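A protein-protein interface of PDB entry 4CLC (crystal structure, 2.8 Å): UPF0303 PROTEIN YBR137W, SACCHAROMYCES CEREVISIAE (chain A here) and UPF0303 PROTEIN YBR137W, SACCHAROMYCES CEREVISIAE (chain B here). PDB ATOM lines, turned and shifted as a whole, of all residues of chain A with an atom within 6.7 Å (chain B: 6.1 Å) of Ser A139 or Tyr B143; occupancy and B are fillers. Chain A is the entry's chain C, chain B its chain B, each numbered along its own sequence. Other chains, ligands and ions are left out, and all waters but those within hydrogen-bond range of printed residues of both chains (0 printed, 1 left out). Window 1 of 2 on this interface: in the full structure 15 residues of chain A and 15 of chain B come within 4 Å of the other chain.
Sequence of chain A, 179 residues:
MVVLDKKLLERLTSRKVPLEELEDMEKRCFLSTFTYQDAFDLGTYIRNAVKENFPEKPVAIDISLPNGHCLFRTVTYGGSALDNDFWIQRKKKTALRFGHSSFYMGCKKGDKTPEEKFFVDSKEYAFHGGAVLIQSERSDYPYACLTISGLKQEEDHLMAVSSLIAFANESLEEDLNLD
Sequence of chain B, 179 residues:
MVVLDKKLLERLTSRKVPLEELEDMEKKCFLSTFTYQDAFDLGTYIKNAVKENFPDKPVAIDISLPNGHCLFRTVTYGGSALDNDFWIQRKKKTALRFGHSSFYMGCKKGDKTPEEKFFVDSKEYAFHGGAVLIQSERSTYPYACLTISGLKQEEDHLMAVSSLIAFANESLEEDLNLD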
ATOM      1  N   GLN A 135      19.972  -6.478 -14.336  1.00  0.00           N
ATOM      2  CA  GLN A 135      19.220  -5.247 -14.200  1.00  0.00           C
ATOM      3  C   GLN A 135      19.844  -4.099 -14.957  1.00  0.00           C
ATOM      4  O   GLN A 135      21.017  -4.127 -15.308  1.00  0.00           O
ATOM      5  CB  GLN A 135      19.057  -4.886 -12.724  1.00  0.00           C
ATOM      6  CG  GLN A 135      18.026  -5.734 -11.992  1.00  0.00           C
ATOM      7  CD  GLN A 135      16.613  -5.481 -12.487  1.00  0.00           C
ATOM      8  OE1 GLN A 135      16.346  -4.502 -13.207  1.00  0.00           O
ATOM      9  NE2 GLN A 135      15.697  -6.361 -12.111  1.00  0.00           N
ATOM     10  N   SER A 136      19.036  -3.090 -15.231  1.00  0.00           N
ATOM     11  CA  SER A 136      19.540  -1.893 -15.869  1.00  0.00           C
ATOM     12  C   SER A 136      19.337  -0.652 -15.025  1.00  0.00           C
ATOM     13  O   SER A 136      18.198  -0.287 -14.702  1.00  0.00           O
ATOM     14  CB  SER A 136      18.863  -1.691 -17.210  1.00  0.00           C
ATOM     15  OG  SER A 136      19.054  -0.371 -17.683  1.00  0.00           O
ATOM     16  N   GLU A 137      20.446  -0.011 -14.674  1.00  0.00           N
ATOM     17  CA  GLU A 137      20.409   1.369 -14.225  1.00  0.00           C
ATOM     18  C   GLU A 137      19.633   2.108 -15.282  1.00  0.00           C
ATOM     19  O   GLU A 137      19.908   1.923 -16.472  1.00  0.00           O
ATOM     20  CB  GLU A 137      21.815   1.950 -14.087  1.00  0.00           C
ATOM     21  CG  GLU A 137      21.884   3.469 -14.068  1.00  0.00           C
ATOM     22  CD  GLU A 137      23.309   3.998 -14.252  1.00  0.00           C
ATOM     23  OE1 GLU A 137      24.198   3.198 -14.640  1.00  0.00           O
ATOM     24  OE2 GLU A 137      23.530   5.215 -14.017  1.00  0.00           O
ATOM     25  N   ARG A 138      18.653   2.896 -14.855  1.00  0.00           N
ATOM     26  CA  ARG A 138      17.796   3.706 -15.744  1.00  0.00           C
ATOM     27  C   ARG A 138      16.639   2.976 -16.446  1.00  0.00           C
ATOM     28  O   ARG A 138      15.737   3.649 -16.958  1.00  0.00           O
ATOM     29  CB  ARG A 138      18.659   4.429 -16.821  1.00  0.00           C
ATOM     30  N   SER A 139      16.633   1.639 -16.496  1.00  0.00           N
ATOM     31  CA  SER A 139      15.523   0.970 -17.204  1.00  0.00           C
ATOM     32  C   SER A 139      14.344   0.415 -16.419  1.00  0.00           C
ATOM     33  O   SER A 139      13.356   0.020 -17.053  1.00  0.00           O
ATOM     34  CB  SER A 139      16.042  -0.190 -18.060  1.00  0.00           C
ATOM     35  OG  SER A 139      14.970  -0.982 -18.564  1.00  0.00           O
ATOM     36  N   ASP A 140      14.435   0.301 -15.097  1.00  0.00           N
ATOM     37  CA  ASP A 140      13.277  -0.174 -14.315  1.00  0.00           C
ATOM     38  C   ASP A 140      12.898  -1.644 -14.637  1.00  0.00           C
ATOM     39  O   ASP A 140      12.223  -2.297 -13.837  1.00  0.00           O
ATOM     40  CB  ASP A 140      12.056   0.745 -14.557  1.00  0.00           C
ATOM     41  CG  ASP A 140      11.305   1.123 -13.272  1.00  0.00           C
ATOM     42  OD1 ASP A 140      11.775   0.792 -12.158  1.00  0.00           O
ATOM     43  OD2 ASP A 140      10.242   1.779 -13.385  1.00  0.00           O
ATOM     44  N   TYR A 141      13.391  -2.163 -15.769  1.00  0.00           N
ATOM     45  CA  TYR A 141      13.107  -3.514 -16.262  1.00  0.00           C
ATOM     46  C   TYR A 141      14.398  -4.113 -16.809  1.00  0.00           C
ATOM     47  O   TYR A 141      15.227  -3.386 -17.345  1.00  0.00           O
ATOM     48  CB  TYR A 141      12.028  -3.494 -17.343  1.00  0.00           C
ATOM     49  CG  TYR A 141      10.760  -2.794 -16.923  1.00  0.00           C
ATOM     50  CD1 TYR A 141       9.802  -3.443 -16.144  1.00  0.00           C
ATOM     51  CD2 TYR A 141      10.522  -1.476 -17.297  1.00  0.00           C
ATOM     52  CE1 TYR A 141       8.651  -2.792 -15.751  1.00  0.00           C
ATOM     53  CE2 TYR A 141       9.369  -0.819 -16.913  1.00  0.00           C
ATOM     54  CZ  TYR A 141       8.441  -1.472 -16.136  1.00  0.00           C
ATOM     55  OH  TYR A 141       7.296  -0.803 -15.758  1.00  0.00           O
ATOM     56  N   PRO A 142      14.564  -5.442 -16.698  1.00  0.00           N
ATOM     57  CA  PRO A 142      15.872  -6.067 -16.882  1.00  0.00           C
ATOM     58  C   PRO A 142      16.417  -5.940 -18.303  1.00  0.00           C
ATOM     59  O   PRO A 142      15.620  -5.956 -19.245  1.00  0.00           O
ATOM     60  CB  PRO A 142      15.597  -7.549 -16.559  1.00  0.00           C
ATOM     61  CG  PRO A 142      14.252  -7.603 -15.978  1.00  0.00           C
ATOM     62  CD  PRO A 142      13.514  -6.458 -16.550  1.00  0.00           C
ATOM     63  N   TYR A 143      17.742  -5.836 -18.449  1.00  0.00           N
ATOM     64  CA  TYR A 143      18.381  -5.966 -19.757  1.00  0.00           C
ATOM     65  C   TYR A 143      18.159  -7.364 -20.295  1.00  0.00           C
ATOM     66  O   TYR A 143      17.797  -7.555 -21.459  1.00  0.00           O
ATOM     67  CB  TYR A 143      19.884  -5.717 -19.692  1.00  0.00           C
ATOM     68  CG  TYR A 143      20.309  -4.273 -19.658  1.00  0.00           C
ATOM     69  CD1 TYR A 143      19.731  -3.331 -20.504  1.00  0.00           C
ATOM     70  CD2 TYR A 143      21.298  -3.853 -18.770  1.00  0.00           C
ATOM     71  CE1 TYR A 143      20.125  -2.021 -20.474  1.00  0.00           C
ATOM     72  CE2 TYR A 143      21.699  -2.547 -18.726  1.00  0.00           C
ATOM     73  CZ  TYR A 143      21.115  -1.627 -19.576  1.00  0.00           C
ATOM     74  OH  TYR A 143      21.516  -0.306 -19.512  1.00  0.00           O
ATOM     75  N   LEU B  31      14.822   6.398 -25.709  1.00  0.00           N
ATOM     76  CA  LEU B  31      14.721   7.133 -24.470  1.00  0.00           C
ATOM     77  C   LEU B  31      15.996   6.880 -23.660  1.00  0.00           C
ATOM     78  O   LEU B  31      16.648   5.827 -23.798  1.00  0.00           O
ATOM     79  CB  LEU B  31      13.477   6.701 -23.701  1.00  0.00           C
ATOM     80  CG  LEU B  31      12.222   6.546 -24.569  1.00  0.00           C
ATOM     81  CD1 LEU B  31      11.086   5.865 -23.795  1.00  0.00           C
ATOM     82  CD2 LEU B  31      11.769   7.889 -25.151  1.00  0.00           C
ATOM     83  N   SER B  32      16.377   7.862 -22.847  1.00  0.00           N
ATOM     84  CA  SER B  32      17.537   7.723 -21.973  1.00  0.00           C
ATOM     85  C   SER B  32      17.177   6.980 -20.689  1.00  0.00           C
ATOM     86  O   SER B  32      18.017   6.312 -20.081  1.00  0.00           O
ATOM     87  CB  SER B  32      18.135   9.094 -21.666  1.00  0.00           C
ATOM     88  OG  SER B  32      18.206   9.917 -22.830  1.00  0.00           O
ATOM     89  N   THR B  33      15.920   7.101 -20.283  1.00  0.00           N
ATOM     90  CA  THR B  33      15.407   6.340 -19.153  1.00  0.00           C
ATOM     91  C   THR B  33      14.102   5.655 -19.542  1.00  0.00           C
ATOM     92  O   THR B  33      13.360   6.160 -20.395  1.00  0.00           O
ATOM     93  CB  THR B  33      15.164   7.234 -17.895  1.00  0.00           C
ATOM     94  OG1 THR B  33      13.902   7.917 -17.999  1.00  0.00           O
ATOM     95  CG2 THR B  33      16.290   8.231 -17.715  1.00  0.00           C
ATOM     96  N   PHE B  34      13.823   4.510 -18.926  1.00  0.00           N
ATOM     97  CA  PHE B  34      12.531   3.859 -19.112  1.00  0.00           C
ATOM     98  C   PHE B  34      11.943   3.391 -17.787  1.00  0.00           C
ATOM     99  O   PHE B  34      12.496   2.509 -17.152  1.00  0.00           O
ATOM    100  CB  PHE B  34      12.664   2.679 -20.074  1.00  0.00           C
ATOM    101  CG  PHE B  34      11.366   2.249 -20.675  1.00  0.00           C
ATOM    102  CD1 PHE B  34      10.664   3.099 -21.515  1.00  0.00           C
ATOM    103  CD2 PHE B  34      10.838   0.996 -20.400  1.00  0.00           C
ATOM    104  CE1 PHE B  34       9.452   2.707 -22.076  1.00  0.00           C
ATOM    105  CE2 PHE B  34       9.636   0.594 -20.957  1.00  0.00           C
ATOM    106  CZ  PHE B  34       8.938   1.452 -21.794  1.00  0.00           C
ATOM    107  N   THR B  35      10.813   3.964 -17.379  1.00  0.00           N
ATOM    108  CA  THR B  35      10.203   3.594 -16.103  1.00  0.00           C
ATOM    109  C   THR B  35       8.752   3.194 -16.267  1.00  0.00           C
ATOM    110  O   THR B  35       8.190   3.341 -17.343  1.00  0.00           O
ATOM    111  CB  THR B  35      10.246   4.757 -15.081  1.00  0.00           C
ATOM    112  OG1 THR B  35       9.402   5.831 -15.536  1.00  0.00           O
ATOM    113  CG2 THR B  35      11.666   5.260 -14.880  1.00  0.00           C
ATOM    114  N   SER B  64       4.404  -2.840 -24.489  1.00  0.00           N
ATOM    115  CA  SER B  64       4.721  -4.017 -23.680  1.00  0.00           C
ATOM    116  C   SER B  64       6.226  -4.254 -23.723  1.00  0.00           C
ATOM    117  O   SER B  64       6.932  -3.574 -24.453  1.00  0.00           O
ATOM    118  CB  SER B  64       3.967  -5.245 -24.183  1.00  0.00           C
ATOM    119  OG  SER B  64       2.563  -5.028 -24.218  1.00  0.00           O
ATOM    120  N   LEU B  65       6.708  -5.260 -23.010  1.00  0.00           N
ATOM    121  CA  LEU B  65       8.142  -5.476 -22.867  1.00  0.00           C
ATOM    122  C   LEU B  65       8.519  -6.725 -23.652  1.00  0.00           C
ATOM    123  O   LEU B  65       7.659  -7.555 -23.937  1.00  0.00           O
ATOM    124  CB  LEU B  65       8.531  -5.645 -21.392  1.00  0.00           C
ATOM    125  CG  LEU B  65       8.235  -4.592 -20.331  1.00  0.00           C
ATOM    126  CD1 LEU B  65       8.705  -5.129 -18.998  1.00  0.00           C
ATOM    127  CD2 LEU B  65       8.908  -3.277 -20.645  1.00  0.00           C
ATOM    128  N   PRO B  66       9.803  -6.870 -24.015  1.00  0.00           N
ATOM    129  CA  PRO B  66      10.191  -7.990 -24.885  1.00  0.00           C
ATOM    130  C   PRO B  66       9.654  -9.360 -24.441  1.00  0.00           C
ATOM    131  O   PRO B  66       9.521 -10.267 -25.275  1.00  0.00           O
ATOM    132  CB  PRO B  66      11.723  -7.964 -24.809  1.00  0.00           C
ATOM    133  CG  PRO B  66      12.044  -6.508 -24.575  1.00  0.00           C
ATOM    134  CD  PRO B  66      10.945  -5.998 -23.689  1.00  0.00           C
ATOM    135  N   ILE B 134      10.917   0.596 -28.960  1.00  0.00           N
ATOM    136  CA  ILE B 134      11.541   1.645 -28.139  1.00  0.00           C
ATOM    137  C   ILE B 134      12.964   1.252 -27.780  1.00  0.00           C
ATOM    138  O   ILE B 134      13.206   0.201 -27.175  1.00  0.00           O
ATOM    139  CB  ILE B 134      10.777   1.912 -26.835  1.00  0.00           C
ATOM    140  CG1 ILE B 134       9.295   2.147 -27.117  1.00  0.00           C
ATOM    141  CG2 ILE B 134      11.364   3.111 -26.123  1.00  0.00           C
ATOM    142  CD1 ILE B 134       8.434   2.068 -25.884  1.00  0.00           C
ATOM    143  N   GLN B 135      13.907   2.112 -28.143  1.00  0.00           N
ATOM    144  CA  GLN B 135      15.308   1.777 -27.993  1.00  0.00           C
ATOM    145  C   GLN B 135      15.938   2.325 -26.712  1.00  0.00           C
ATOM    146  O   GLN B 135      15.282   2.953 -25.886  1.00  0.00           O
ATOM    147  CB  GLN B 135      16.086   2.258 -29.217  1.00  0.00           C
ATOM    148  CG  GLN B 135      15.716   1.540 -30.511  1.00  0.00           C
ATOM    149  CD  GLN B 135      16.041   0.071 -30.451  1.00  0.00           C
ATOM    150  OE1 GLN B 135      16.675  -0.399 -29.500  1.00  0.00           O
ATOM    151  NE2 GLN B 135      15.623  -0.670 -31.469  1.00  0.00           N
ATOM    152  N   SER B 136      17.217   2.033 -26.546  1.00  0.00           N
ATOM    153  CA  SER B 136      17.945   2.361 -25.335  1.00  0.00           C
ATOM    154  C   SER B 136      19.286   2.935 -25.723  1.00  0.00           C
ATOM    155  O   SER B 136      20.065   2.267 -26.408  1.00  0.00           O
ATOM    156  CB  SER B 136      18.131   1.121 -24.453  1.00  0.00           C
ATOM    157  OG  SER B 136      19.205   1.277 -23.540  1.00  0.00           O
ATOM    158  N   GLU B 137      19.548   4.169 -25.299  1.00  0.00           N
ATOM    159  CA  GLU B 137      20.828   4.806 -25.557  1.00  0.00           C
ATOM    160  C   GLU B 137      21.942   3.883 -25.115  1.00  0.00           C
ATOM    161  O   GLU B 137      22.943   3.731 -25.804  1.00  0.00           O
ATOM    162  CB  GLU B 137      20.927   6.159 -24.836  1.00  0.00           C
ATOM    163  N   ARG B 138      21.754   3.238 -23.975  1.00  0.00           N
ATOM    164  CA  ARG B 138      22.830   2.454 -23.386  1.00  0.00           C
ATOM    165  C   ARG B 138      22.927   0.991 -23.871  1.00  0.00           C
ATOM    166  O   ARG B 138      23.949   0.341 -23.653  1.00  0.00           O
ATOM    167  CB  ARG B 138      22.697   2.492 -21.870  1.00  0.00           C
ATOM    168  N   SER B 139      21.892   0.476 -24.537  1.00  0.00           N
ATOM    169  CA  SER B 139      21.891  -0.931 -24.969  1.00  0.00           C
ATOM    170  C   SER B 139      21.719  -1.144 -26.475  1.00  0.00           C
ATOM    171  O   SER B 139      21.004  -0.377 -27.143  1.00  0.00           O
ATOM    172  CB  SER B 139      20.782  -1.703 -24.244  1.00  0.00           C
ATOM    173  OG  SER B 139      20.771  -3.064 -24.651  1.00  0.00           O
ATOM    174  N   TYR B 141      20.060  -3.493 -27.452  1.00  0.00           N
ATOM    175  CA  TYR B 141      18.765  -4.188 -27.491  1.00  0.00           C
ATOM    176  C   TYR B 141      17.677  -3.278 -26.885  1.00  0.00           C
ATOM    177  O   TYR B 141      17.997  -2.376 -26.102  1.00  0.00           O
ATOM    178  CB  TYR B 141      18.886  -5.529 -26.770  1.00  0.00           C
ATOM    179  CG  TYR B 141      20.137  -6.260 -27.184  1.00  0.00           C
ATOM    180  CD1 TYR B 141      20.186  -6.980 -28.377  1.00  0.00           C
ATOM    181  CD2 TYR B 141      21.293  -6.186 -26.419  1.00  0.00           C
ATOM    182  CE1 TYR B 141      21.334  -7.620 -28.776  1.00  0.00           C
ATOM    183  CE2 TYR B 141      22.446  -6.833 -26.812  1.00  0.00           C
ATOM    184  CZ  TYR B 141      22.457  -7.535 -27.990  1.00  0.00           C
ATOM    185  OH  TYR B 141      23.601  -8.164 -28.373  1.00  0.00           O
ATOM    186  N   PRO B 142      16.401  -3.464 -27.295  1.00  0.00           N
ATOM    187  CA  PRO B 142      15.324  -2.516 -26.977  1.00  0.00           C
ATOM    188  C   PRO B 142      14.674  -2.663 -25.599  1.00  0.00           C
ATOM    189  O   PRO B 142      14.559  -3.767 -25.067  1.00  0.00           O
ATOM    190  CB  PRO B 142      14.303  -2.796 -28.074  1.00  0.00           C
ATOM    191  CG  PRO B 142      14.453  -4.235 -28.329  1.00  0.00           C
ATOM    192  CD  PRO B 142      15.898  -4.594 -28.088  1.00  0.00           C
ATOM    193  N   TYR B 143      14.202  -1.544 -25.065  1.00  0.00           N
ATOM    194  CA  TYR B 143      13.487  -1.505 -23.787  1.00  0.00           C
ATOM    195  C   TYR B 143      12.203  -2.276 -23.871  1.00  0.00           C
ATOM    196  O   TYR B 143      11.947  -3.182 -23.088  1.00  0.00           O
ATOM    197  CB  TYR B 143      13.145  -0.061 -23.382  1.00  0.00           C
ATOM    198  CG  TYR B 143      14.267   0.703 -22.732  1.00  0.00           C
ATOM    199  CD1 TYR B 143      15.218   0.043 -21.957  1.00  0.00           C
ATOM    200  CD2 TYR B 143      14.383   2.079 -22.895  1.00  0.00           C
ATOM    201  CE1 TYR B 143      16.247   0.727 -21.348  1.00  0.00           C
ATOM    202  CE2 TYR B 143      15.408   2.779 -22.288  1.00  0.00           C
ATOM    203  CZ  TYR B 143      16.342   2.095 -21.513  1.00  0.00           C
ATOM    204  OH  TYR B 143      17.386   2.764 -20.900  1.00  0.00           O
ATOM    205  N   ALA B 144      11.391  -1.877 -24.840  1.00  0.00           N
ATOM    206  CA  ALA B 144      10.016  -2.318 -24.949  1.00  0.00           C
ATOM    207  C   ALA B 144       9.568  -2.216 -26.388  1.00  0.00           C
ATOM    208  O   ALA B 144      10.376  -1.987 -27.287  1.00  0.00           O
ATOM    209  CB  ALA B 144       9.139  -1.491 -24.069  1.00  0.00           C
ATOM    210  N   CYS B 145       8.276  -2.393 -26.606  1.00  0.00           N
ATOM    211  CA  CYS B 145       7.719  -2.241 -27.939  1.00  0.00           C
ATOM    212  C   CYS B 145       6.471  -1.370 -27.893  1.00  0.00           C
ATOM    213  O   CYS B 145       5.606  -1.531 -27.016  1.00  0.00           O
ATOM    214  CB  CYS B 145       7.401  -3.613 -28.558  1.00  0.00           C
ATOM    215  SG  CYS B 145       6.715  -3.565 -30.264  1.00  0.00           S
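N of Phe B34 is in hydrogen-bond range of O of Arg A138, at 2.9 Å.
O of Phe B34 lies close to O of Ser A139 (2.6 Å).
O of Ile B134 is in hydrogen-bond range of N of Tyr B143.
The backbone NH of Arg B138 lies close to the side-chain hydroxyl of Ser B136 (3.2 Å).
The side-chain hydroxyl of Ser B136 lies within hydrogen-bond range of the backbone NH of Ser B139 (3.0 Å).
The backbone NH (N) of Tyr B141 lies within hydrogen-bond range of the side-chain hydroxyl (OG) of Ser B139 (2.9 Å).
The backbone NH of Ser A139 sits close to the side-chain hydroxyl of Ser A136 (3.4 Å).
OH of Tyr A143 sits close to OG of Ser A136 (3.1 Å).
Among the printed residues, pairs that only touch across the chains: Arg A138 with Ser B32 (3.8 Å), Arg A138 with Thr B33 (3.5 Å), Ser A139 with Tyr B143 (3.4 Å), Asp A140 with Phe B34 (3.2 Å), Asp A140 with Thr B35 (3.3 Å), Tyr A141 with Phe B34 (3.98 Å), Tyr A141 with Leu B65 (3.5 Å), Tyr A143 with Arg B138 (3.8 Å) and Tyr A143 with Ser B139 (3.8 Å).
Printed residues of chain B within 4 Å of Tyr A141: Phe B34 and Leu B65.
Of the printed residues of chain B, Tyr A143 touches Arg B138 (3.8 Å) and Ser B139 (3.8 Å).
Of the printed residues of chain A, Ser B32 touches Arg A138.
Printed residues of chain A within 4 Å of Thr B33: Arg A138.
Printed residues of chain A within 4 Å of Arg B138: Tyr A143.
Pro B142 touches none of the printed residues of chain A.
Of chain A, only Ser A139 comes within 4 Å of Tyr B143.
The nearest printed residue of chain A that does not touch Thr B35 is Tyr A141 (4.1 Å).
Of the 19 printed residues of chain B, 8 touch a printed residue of chain A.
Hydrophobic or aromatic side chains of chain B within 4 Å of the printed part of chain A: Phe B34, Leu B65 and Tyr B143.
Along chain B the printed residues that touch a printed residue of chain A span positions 32 to 143.
Of the 9 printed residues of chain A, 5 touch a printed residue of chain B.
Printed residues of chain A that touch a printed residue of chain B: Arg A138, Ser A139, Asp A140, Tyr A141 and Tyr A143.
Hydrophobic or aromatic side chains of chain A within 4 Å of the printed part of chain B: Tyr A141 and Tyr A143.
Among the printed residues, no Asp or Glu carboxylate lies within 4 Å of a Lys or Arg side-chain nitrogen of the other chain.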
